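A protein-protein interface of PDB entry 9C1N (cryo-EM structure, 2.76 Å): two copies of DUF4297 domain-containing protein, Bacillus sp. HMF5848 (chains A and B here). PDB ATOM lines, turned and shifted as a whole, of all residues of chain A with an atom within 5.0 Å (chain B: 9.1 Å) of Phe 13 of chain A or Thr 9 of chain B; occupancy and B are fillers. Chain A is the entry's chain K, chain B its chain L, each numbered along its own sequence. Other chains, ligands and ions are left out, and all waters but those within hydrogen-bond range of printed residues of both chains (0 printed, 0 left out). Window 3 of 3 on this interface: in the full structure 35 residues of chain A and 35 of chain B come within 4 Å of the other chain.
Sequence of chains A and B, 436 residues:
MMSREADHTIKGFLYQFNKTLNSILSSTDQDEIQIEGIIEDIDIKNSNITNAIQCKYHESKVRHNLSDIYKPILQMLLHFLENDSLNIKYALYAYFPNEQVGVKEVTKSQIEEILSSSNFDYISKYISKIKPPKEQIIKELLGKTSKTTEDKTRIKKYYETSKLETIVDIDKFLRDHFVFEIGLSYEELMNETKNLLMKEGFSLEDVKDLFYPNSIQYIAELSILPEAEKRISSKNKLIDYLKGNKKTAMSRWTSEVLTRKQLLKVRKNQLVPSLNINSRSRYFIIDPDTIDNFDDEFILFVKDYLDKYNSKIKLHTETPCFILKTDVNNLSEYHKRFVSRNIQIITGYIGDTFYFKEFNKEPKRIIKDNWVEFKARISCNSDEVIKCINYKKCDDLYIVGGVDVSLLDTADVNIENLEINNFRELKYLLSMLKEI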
ATOM      1  N   THR A   9      16.216  24.176  16.626  1.00  0.00           N
ATOM      2  CA  THR A   9      14.860  24.699  16.767  1.00  0.00           C
ATOM      3  C   THR A   9      14.610  25.210  18.182  1.00  0.00           C
ATOM      4  O   THR A   9      13.955  26.243  18.369  1.00  0.00           O
ATOM      5  CB  THR A   9      13.840  23.621  16.398  1.00  0.00           C
ATOM      6  OG1 THR A   9      14.242  22.980  15.180  1.00  0.00           O
ATOM      7  CG2 THR A   9      12.465  24.238  16.201  1.00  0.00           C
ATOM      8  N   ILE A  10      15.124  24.501  19.189  1.00  0.00           N
ATOM      9  CA  ILE A  10      14.982  24.952  20.571  1.00  0.00           C
ATOM     10  C   ILE A  10      15.692  26.285  20.771  1.00  0.00           C
ATOM     11  O   ILE A  10      15.163  27.198  21.417  1.00  0.00           O
ATOM     12  CB  ILE A  10      15.511  23.879  21.540  1.00  0.00           C
ATOM     13  CG1 ILE A  10      14.685  22.597  21.424  1.00  0.00           C
ATOM     14  CG2 ILE A  10      15.497  24.396  22.971  1.00  0.00           C
ATOM     15  CD1 ILE A  10      15.343  21.390  22.052  1.00  0.00           C
ATOM     16  N   LYS A  11      16.901  26.416  20.220  1.00  0.00           N
ATOM     17  CA  LYS A  11      17.636  27.671  20.340  1.00  0.00           C
ATOM     18  C   LYS A  11      16.913  28.803  19.621  1.00  0.00           C
ATOM     19  O   LYS A  11      16.880  29.936  20.109  1.00  0.00           O
ATOM     20  CB  LYS A  11      19.056  27.505  19.797  1.00  0.00           C
ATOM     21  CG  LYS A  11      20.027  28.568  20.281  1.00  0.00           C
ATOM     22  CD  LYS A  11      21.463  28.203  19.941  1.00  0.00           C
ATOM     23  CE  LYS A  11      22.441  29.201  20.540  1.00  0.00           C
ATOM     24  NZ  LYS A  11      23.856  28.792  20.321  1.00  0.00           N
ATOM     25  N   GLY A  12      16.326  28.514  18.458  1.00  0.00           N
ATOM     26  CA  GLY A  12      15.563  29.532  17.754  1.00  0.00           C
ATOM     27  C   GLY A  12      14.334  29.978  18.524  1.00  0.00           C
ATOM     28  O   GLY A  12      14.013  31.168  18.564  1.00  0.00           O
ATOM     29  N   PHE A  13      13.629  29.030  19.144  1.00  0.00           N
ATOM     30  CA  PHE A  13      12.469  29.390  19.954  1.00  0.00           C
ATOM     31  C   PHE A  13      12.879  30.197  21.181  1.00  0.00           C
ATOM     32  O   PHE A  13      12.186  31.147  21.568  1.00  0.00           O
ATOM     33  CB  PHE A  13      11.700  28.134  20.361  1.00  0.00           C
ATOM     34  CG  PHE A  13      10.690  27.690  19.344  1.00  0.00           C
ATOM     35  CD1 PHE A  13       9.679  28.545  18.935  1.00  0.00           C
ATOM     36  CD2 PHE A  13      10.753  26.423  18.790  1.00  0.00           C
ATOM     37  CE1 PHE A  13       8.749  28.143  17.996  1.00  0.00           C
ATOM     38  CE2 PHE A  13       9.825  26.016  17.851  1.00  0.00           C
ATOM     39  CZ  PHE A  13       8.822  26.875  17.454  1.00  0.00           C
ATOM     40  N   LEU A  14      14.003  29.837  21.806  1.00  0.00           N
ATOM     41  CA  LEU A  14      14.509  30.626  22.925  1.00  0.00           C
ATOM     42  C   LEU A  14      14.891  32.031  22.478  1.00  0.00           C
ATOM     43  O   LEU A  14      14.655  33.007  23.199  1.00  0.00           O
ATOM     44  CB  LEU A  14      15.703  29.921  23.569  1.00  0.00           C
ATOM     45  CG  LEU A  14      15.378  28.722  24.462  1.00  0.00           C
ATOM     46  CD1 LEU A  14      16.652  28.110  25.024  1.00  0.00           C
ATOM     47  CD2 LEU A  14      14.434  29.126  25.584  1.00  0.00           C
ATOM     48  N   TYR A  15      15.486  32.152  21.289  1.00  0.00           N
ATOM     49  CA  TYR A  15      15.812  33.465  20.742  1.00  0.00           C
ATOM     50  C   TYR A  15      14.552  34.286  20.494  1.00  0.00           C
ATOM     51  O   TYR A  15      14.527  35.492  20.758  1.00  0.00           O
ATOM     52  CB  TYR A  15      16.613  33.305  19.451  1.00  0.00           C
ATOM     53  CG  TYR A  15      17.176  34.598  18.908  1.00  0.00           C
ATOM     54  CD1 TYR A  15      18.303  35.178  19.474  1.00  0.00           C
ATOM     55  CD2 TYR A  15      16.580  35.239  17.829  1.00  0.00           C
ATOM     56  CE1 TYR A  15      18.822  36.358  18.980  1.00  0.00           C
ATOM     57  CE2 TYR A  15      17.091  36.420  17.329  1.00  0.00           C
ATOM     58  CZ  TYR A  15      18.212  36.976  17.909  1.00  0.00           C
ATOM     59  OH  TYR A  15      18.726  38.153  17.415  1.00  0.00           O
ATOM     60  N   GLN A  16      13.502  33.648  19.972  1.00  0.00           N
ATOM     61  CA  GLN A  16      12.238  34.346  19.762  1.00  0.00           C
ATOM     62  C   GLN A  16      11.642  34.815  21.085  1.00  0.00           C
ATOM     63  O   GLN A  16      11.130  35.938  21.183  1.00  0.00           O
ATOM     64  CB  GLN A  16      11.255  33.440  19.023  1.00  0.00           C
ATOM     65  CG  GLN A  16       9.872  34.044  18.837  1.00  0.00           C
ATOM     66  CD  GLN A  16       8.892  33.074  18.208  1.00  0.00           C
ATOM     67  OE1 GLN A  16       9.285  32.151  17.494  1.00  0.00           O
ATOM     68  NE2 GLN A  16       7.607  33.278  18.472  1.00  0.00           N
ATOM     69  N   PHE A  17      11.696  33.965  22.113  1.00  0.00           N
ATOM     70  CA  PHE A  17      11.199  34.361  23.428  1.00  0.00           C
ATOM     71  C   PHE A  17      12.001  35.526  23.993  1.00  0.00           C
ATOM     72  O   PHE A  17      11.435  36.457  24.579  1.00  0.00           O
ATOM     73  CB  PHE A  17      11.240  33.170  24.388  1.00  0.00           C
ATOM     74  CG  PHE A  17      10.342  32.036  23.987  1.00  0.00           C
ATOM     75  CD1 PHE A  17       9.227  32.262  23.196  1.00  0.00           C
ATOM     76  CD2 PHE A  17      10.615  30.742  24.399  1.00  0.00           C
ATOM     77  CE1 PHE A  17       8.401  31.220  22.827  1.00  0.00           C
ATOM     78  CE2 PHE A  17       9.792  29.696  24.032  1.00  0.00           C
ATOM     79  CZ  PHE A  17       8.684  29.936  23.245  1.00  0.00           C
ATOM     80  N   GLU A  36       3.252  35.518  20.278  1.00  0.00           N
ATOM     81  CA  GLU A  36       2.770  34.614  19.235  1.00  0.00           C
ATOM     82  C   GLU A  36       1.478  35.154  18.624  1.00  0.00           C
ATOM     83  O   GLU A  36       0.435  34.499  18.606  1.00  0.00           O
ATOM     84  CB  GLU A  36       2.585  33.194  19.776  1.00  0.00           C
ATOM     85  CG  GLU A  36       3.883  32.421  19.943  1.00  0.00           C
ATOM     86  CD  GLU A  36       4.503  32.030  18.615  1.00  0.00           C
ATOM     87  OE1 GLU A  36       3.754  31.894  17.624  1.00  0.00           O
ATOM     88  OE2 GLU A  36       5.738  31.863  18.562  1.00  0.00           O
ATOM     89  N   ASP B   7       2.272  27.831  17.956  1.00  0.00           N
ATOM     90  CA  ASP B   7       2.024  27.589  19.373  1.00  0.00           C
ATOM     91  C   ASP B   7       2.089  26.100  19.697  1.00  0.00           C
ATOM     92  O   ASP B   7       2.495  25.711  20.791  1.00  0.00           O
ATOM     93  CB  ASP B   7       0.665  28.160  19.783  1.00  0.00           C
ATOM     94  CG  ASP B   7      -0.482  27.569  18.987  1.00  0.00           C
ATOM     95  OD1 ASP B   7      -0.266  27.208  17.811  1.00  0.00           O
ATOM     96  OD2 ASP B   7      -1.598  27.463  19.537  1.00  0.00           O
ATOM     97  N   HIS B   8       1.679  25.270  18.734  1.00  0.00           N
ATOM     98  CA  HIS B   8       1.701  23.825  18.943  1.00  0.00           C
ATOM     99  C   HIS B   8       3.126  23.308  19.104  1.00  0.00           C
ATOM    100  O   HIS B   8       3.388  22.453  19.958  1.00  0.00           O
ATOM    101  CB  HIS B   8       0.998  23.118  17.786  1.00  0.00           C
ATOM    102  CG  HIS B   8      -0.490  23.291  17.788  1.00  0.00           C
ATOM    103  ND1 HIS B   8      -1.273  22.988  18.880  1.00  0.00           N
ATOM    104  CD2 HIS B   8      -1.336  23.740  16.830  1.00  0.00           C
ATOM    105  CE1 HIS B   8      -2.537  23.241  18.596  1.00  0.00           C
ATOM    106  NE2 HIS B   8      -2.603  23.698  17.359  1.00  0.00           N
ATOM    107  N   THR B   9       4.060  23.812  18.293  1.00  0.00           N
ATOM    108  CA  THR B   9       5.453  23.392  18.423  1.00  0.00           C
ATOM    109  C   THR B   9       6.041  23.833  19.759  1.00  0.00           C
ATOM    110  O   THR B   9       6.795  23.084  20.391  1.00  0.00           O
ATOM    111  CB  THR B   9       6.280  23.947  17.263  1.00  0.00           C
ATOM    112  OG1 THR B   9       5.600  23.696  16.027  1.00  0.00           O
ATOM    113  CG2 THR B   9       7.647  23.282  17.221  1.00  0.00           C
ATOM    114  N   ILE B  10       5.706  25.046  20.204  1.00  0.00           N
ATOM    115  CA  ILE B  10       6.176  25.523  21.502  1.00  0.00           C
ATOM    116  C   ILE B  10       5.619  24.653  22.620  1.00  0.00           C
ATOM    117  O   ILE B  10       6.330  24.303  23.570  1.00  0.00           O
ATOM    118  CB  ILE B  10       5.802  27.003  21.696  1.00  0.00           C
ATOM    119  CG1 ILE B  10       6.463  27.866  20.621  1.00  0.00           C
ATOM    120  CG2 ILE B  10       6.215  27.480  23.078  1.00  0.00           C
ATOM    121  CD1 ILE B  10       5.933  29.279  20.563  1.00  0.00           C
ATOM    122  N   LYS B  11       4.334  24.296  22.529  1.00  0.00           N
ATOM    123  CA  LYS B  11       3.735  23.433  23.541  1.00  0.00           C
ATOM    124  C   LYS B  11       4.383  22.055  23.544  1.00  0.00           C
ATOM    125  O   LYS B  11       4.605  21.469  24.609  1.00  0.00           O
ATOM    126  CB  LYS B  11       2.228  23.319  23.310  1.00  0.00           C
ATOM    127  CG  LYS B  11       1.444  22.922  24.550  1.00  0.00           C
ATOM    128  CD  LYS B  11      -0.043  23.180  24.375  1.00  0.00           C
ATOM    129  CE  LYS B  11      -0.796  22.956  25.675  1.00  0.00           C
ATOM    130  NZ  LYS B  11      -2.238  23.305  25.549  1.00  0.00           N
ATOM    131  N   GLY B  12       4.698  21.522  22.361  1.00  0.00           N
ATOM    132  CA  GLY B  12       5.387  20.243  22.299  1.00  0.00           C
ATOM    133  C   GLY B  12       6.776  20.296  22.905  1.00  0.00           C
ATOM    134  O   GLY B  12       7.194  19.373  23.609  1.00  0.00           O
ATOM    135  N   PHE B  13       7.512  21.378  22.640  1.00  0.00           N
ATOM    136  CA  PHE B  13       8.836  21.532  23.234  1.00  0.00           C
ATOM    137  C   PHE B  13       8.750  21.664  24.750  1.00  0.00           C
ATOM    138  O   PHE B  13       9.573  21.098  25.480  1.00  0.00           O
ATOM    139  CB  PHE B  13       9.551  22.737  22.624  1.00  0.00           C
ATOM    140  CG  PHE B  13      10.291  22.422  21.356  1.00  0.00           C
ATOM    141  CD1 PHE B  13      11.140  21.329  21.289  1.00  0.00           C
ATOM    142  CD2 PHE B  13      10.136  23.214  20.232  1.00  0.00           C
ATOM    143  CE1 PHE B  13      11.821  21.034  20.124  1.00  0.00           C
ATOM    144  CE2 PHE B  13      10.815  22.924  19.064  1.00  0.00           C
ATOM    145  CZ  PHE B  13      11.659  21.832  19.010  1.00  0.00           C
ATOM    146  N   LEU B  14       7.759  22.410  25.244  1.00  0.00           N
ATOM    147  CA  LEU B  14       7.571  22.526  26.686  1.00  0.00           C
ATOM    148  C   LEU B  14       7.193  21.183  27.300  1.00  0.00           C
ATOM    149  O   LEU B  14       7.630  20.853  28.407  1.00  0.00           O
ATOM    150  CB  LEU B  14       6.509  23.580  26.998  1.00  0.00           C
ATOM    151  CG  LEU B  14       6.953  25.038  26.862  1.00  0.00           C
ATOM    152  CD1 LEU B  14       5.809  25.981  27.193  1.00  0.00           C
ATOM    153  CD2 LEU B  14       8.157  25.318  27.749  1.00  0.00           C
ATOM    154  N   TYR B  15       6.374  20.397  26.597  1.00  0.00           N
ATOM    155  CA  TYR B  15       6.032  19.060  27.070  1.00  0.00           C
ATOM    156  C   TYR B  15       7.264  18.167  27.132  1.00  0.00           C
ATOM    157  O   TYR B  15       7.435  17.398  28.084  1.00  0.00           O
ATOM    158  CB  TYR B  15       4.966  18.444  26.164  1.00  0.00           C
ATOM    159  CG  TYR B  15       4.377  17.159  26.694  1.00  0.00           C
ATOM    160  CD1 TYR B  15       3.426  17.174  27.705  1.00  0.00           C
ATOM    161  CD2 TYR B  15       4.770  15.929  26.183  1.00  0.00           C
ATOM    162  CE1 TYR B  15       2.883  16.003  28.192  1.00  0.00           C
ATOM    163  CE2 TYR B  15       4.233  14.751  26.664  1.00  0.00           C
ATOM    164  CZ  TYR B  15       3.290  14.793  27.669  1.00  0.00           C
ATOM    165  OH  TYR B  15       2.751  13.624  28.153  1.00  0.00           O
ATOM    166  N   GLN B  16       8.131  18.252  26.120  1.00  0.00           N
ATOM    167  CA  GLN B  16       9.371  17.483  26.138  1.00  0.00           C
ATOM    168  C   GLN B  16      10.262  17.901  27.302  1.00  0.00           C
ATOM    169  O   GLN B  16      10.858  17.053  27.977  1.00  0.00           O
ATOM    170  CB  GLN B  16      10.110  17.650  24.810  1.00  0.00           C
ATOM    171  CG  GLN B  16      11.441  16.920  24.740  1.00  0.00           C
ATOM    172  CD  GLN B  16      12.178  17.176  23.440  1.00  0.00           C
ATOM    173  OE1 GLN B  16      11.565  17.472  22.414  1.00  0.00           O
ATOM    174  NE2 GLN B  16      13.500  17.067  23.477  1.00  0.00           N
ATOM    175  N   PHE B  17      10.364  19.210  27.550  1.00  0.00           N
ATOM    176  CA  PHE B  17      11.160  19.694  28.676  1.00  0.00           C
ATOM    177  C   PHE B  17      10.590  19.207  30.003  1.00  0.00           C
ATOM    178  O   PHE B  17      11.338  18.806  30.902  1.00  0.00           O
ATOM    179  CB  PHE B  17      11.231  21.220  28.650  1.00  0.00           C
ATOM    180  CG  PHE B  17      11.971  21.775  27.467  1.00  0.00           C
ATOM    181  CD1 PHE B  17      12.902  21.004  26.790  1.00  0.00           C
ATOM    182  CD2 PHE B  17      11.733  23.067  27.029  1.00  0.00           C
ATOM    183  CE1 PHE B  17      13.582  21.513  25.701  1.00  0.00           C
ATOM    184  CE2 PHE B  17      12.410  23.581  25.941  1.00  0.00           C
ATOM    185  CZ  PHE B  17      13.335  22.803  25.276  1.00  0.00           C
ATOM    186  N   TYR B  57       3.865  15.367  21.067  1.00  0.00           N
ATOM    187  CA  TYR B  57       2.680  16.047  21.578  1.00  0.00           C
ATOM    188  C   TYR B  57       1.642  16.112  20.468  1.00  0.00           C
ATOM    189  O   TYR B  57       1.920  16.640  19.386  1.00  0.00           O
ATOM    190  CB  TYR B  57       3.029  17.448  22.084  1.00  0.00           C
ATOM    191  CG  TYR B  57       2.029  18.016  23.066  1.00  0.00           C
ATOM    192  CD1 TYR B  57       1.867  17.451  24.325  1.00  0.00           C
ATOM    193  CD2 TYR B  57       1.254  19.121  22.740  1.00  0.00           C
ATOM    194  CE1 TYR B  57       0.957  17.966  25.228  1.00  0.00           C
ATOM    195  CE2 TYR B  57       0.343  19.644  23.637  1.00  0.00           C
ATOM    196  CZ  TYR B  57       0.198  19.062  24.879  1.00  0.00           C
ATOM    197  OH  TYR B  57      -0.709  19.581  25.774  1.00  0.00           O
ATOM    198  N   GLU B  59      -1.942  17.081  21.008  1.00  0.00           N
ATOM    199  CA  GLU B  59      -3.161  17.593  21.629  1.00  0.00           C
ATOM    200  C   GLU B  59      -4.247  17.878  20.599  1.00  0.00           C
ATOM    201  O   GLU B  59      -5.440  17.782  20.912  1.00  0.00           O
ATOM    202  CB  GLU B  59      -2.848  18.857  22.431  1.00  0.00           C
ATOM    203  CG  GLU B  59      -4.006  19.377  23.267  1.00  0.00           C
ATOM    204  CD  GLU B  59      -3.644  20.623  24.050  1.00  0.00           C
ATOM    205  OE1 GLU B  59      -2.793  21.401  23.571  1.00  0.00           O
ATOM    206  OE2 GLU B  59      -4.212  20.825  25.144  1.00  0.00           O
ATOM    207  N   SER B  60      -3.862  18.221  19.371  1.00  0.00           N
ATOM    208  CA  SER B  60      -4.822  18.576  18.333  1.00  0.00           C
ATOM    209  C   SER B  60      -5.407  17.365  17.618  1.00  0.00           C
ATOM    210  O   SER B  60      -6.255  17.541  16.735  1.00  0.00           O
ATOM    211  CB  SER B  60      -4.167  19.508  17.311  1.00  0.00           C
ATOM    212  OG  SER B  60      -3.066  18.880  16.679  1.00  0.00           O
ATOM    213  N   ALA B 220      16.178  24.037  29.236  1.00  0.00           N
ATOM    214  CA  ALA B 220      16.246  24.708  27.940  1.00  0.00           C
ATOM    215  C   ALA B 220      17.677  25.096  27.590  1.00  0.00           C
ATOM    216  O   ALA B 220      18.101  24.954  26.436  1.00  0.00           O
ATOM    217  CB  ALA B 220      15.340  25.939  27.941  1.00  0.00           C
ATOM    218  N   ILE B 224      20.216  23.408  24.211  1.00  0.00           N
ATOM    219  CA  ILE B 224      20.777  24.110  23.060  1.00  0.00           C
ATOM    220  C   ILE B 224      22.288  23.970  22.954  1.00  0.00           C
ATOM    221  O   ILE B 224      22.885  24.506  22.011  1.00  0.00           O
ATOM    222  CB  ILE B 224      20.408  25.608  23.095  1.00  0.00           C
ATOM    223  CG1 ILE B 224      21.126  26.309  24.250  1.00  0.00           C
ATOM    224  CG2 ILE B 224      18.905  25.780  23.223  1.00  0.00           C
ATOM    225  CD1 ILE B 224      21.094  27.819  24.161  1.00  0.00           C
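Printed residues of chain A that touch a printed residue of chain B: Thr 9, Ile 10, Lys 11, Phe 13, Leu 14, Phe 17 and Glu 36. Hydrophobic or aromatic side chains of chain A within 4 Å of the printed part of chain B: Ile 10, Phe 13, Leu 14 and Phe 17. Of the 16 printed residues of chain B, 6 touch a printed residue of chain A. Among the printed residues, 12 pairs touch across the chains. Among the printed residues, no Asp or Glu carboxylate lies within 4 Å of a Lys or Arg side-chain nitrogen of the other chain.
Thr 9 of chain A touches Phe 13 of chain B, and with the chains exchanged Phe 13 of chain A touches Thr 9 of chain B. Ile 10 of chain A touches Phe 13 of chain B, and with the chains exchanged Phe 13 of chain A touches Ile 10 of chain B. Ile 10 of chain A touches Phe 17 of chain B, and with the chains exchanged Phe 17 of chain A touches Ile 10 of chain B. Phe 13 of chain B touches its own counterpart, Phe 13 of chain A.
CG2 of Thr 9 of chain A touches CE2 of Phe 13 of chain B (3.6 Å). Ile 10 of chain A touches Phe 13 of chain B (CG1 to CE1, 3.5 Å). Ile 10 of chain A touches Phe 17 of chain B. CG2 of Ile 10 of chain A touches CG2 of Ile 224 of chain B, 3.7 Å away. Thr 9 of chain B touches Phe 13 of chain A. CE1 of Phe 13 of chain A touches CG1 of Ile 10 of chain B (3.5 Å). Phe 13 of chain A touches Phe 13 of chain B. Leu 14 of chain A touches Ala 220 of chain B (CD1 to O, 3.7 Å). CD1 of Leu 14 of chain A touches CG2 of Ile 224 of chain B (3.7 Å). OE2 of Glu 36 of chain A touches CD1 of Ile 10 of chain B, at 3.3 Å.
Printed residues of chain B within 4 Å of Phe 13 of chain A: Thr 9, Ile 10 and Phe 13. Thr 9 of chain B touches one residue of chain A. No residue of chain B comes within 4 Å of Gly 12 of chain A. Of the printed residues of chain A, Phe 17 of chain B touches Ile 10 (3.5 Å). Printed residues of chain B within 4 Å of Thr 9 of chain A: Phe 13 (3.6 Å). Of the printed residues of chain A, Ile 224 of chain B touches Ile 10, Lys 11 and Leu 14. Glu 59 of chain B touches none of the printed residues of chain A. The nearest residue of chain B that does not touch Phe 13 of chain A is Asp 7 of chain B (6.5 Å). The nearest printed residue of chain A that does not touch Thr 9 of chain B is Thr 9 of chain A (5.0 Å).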
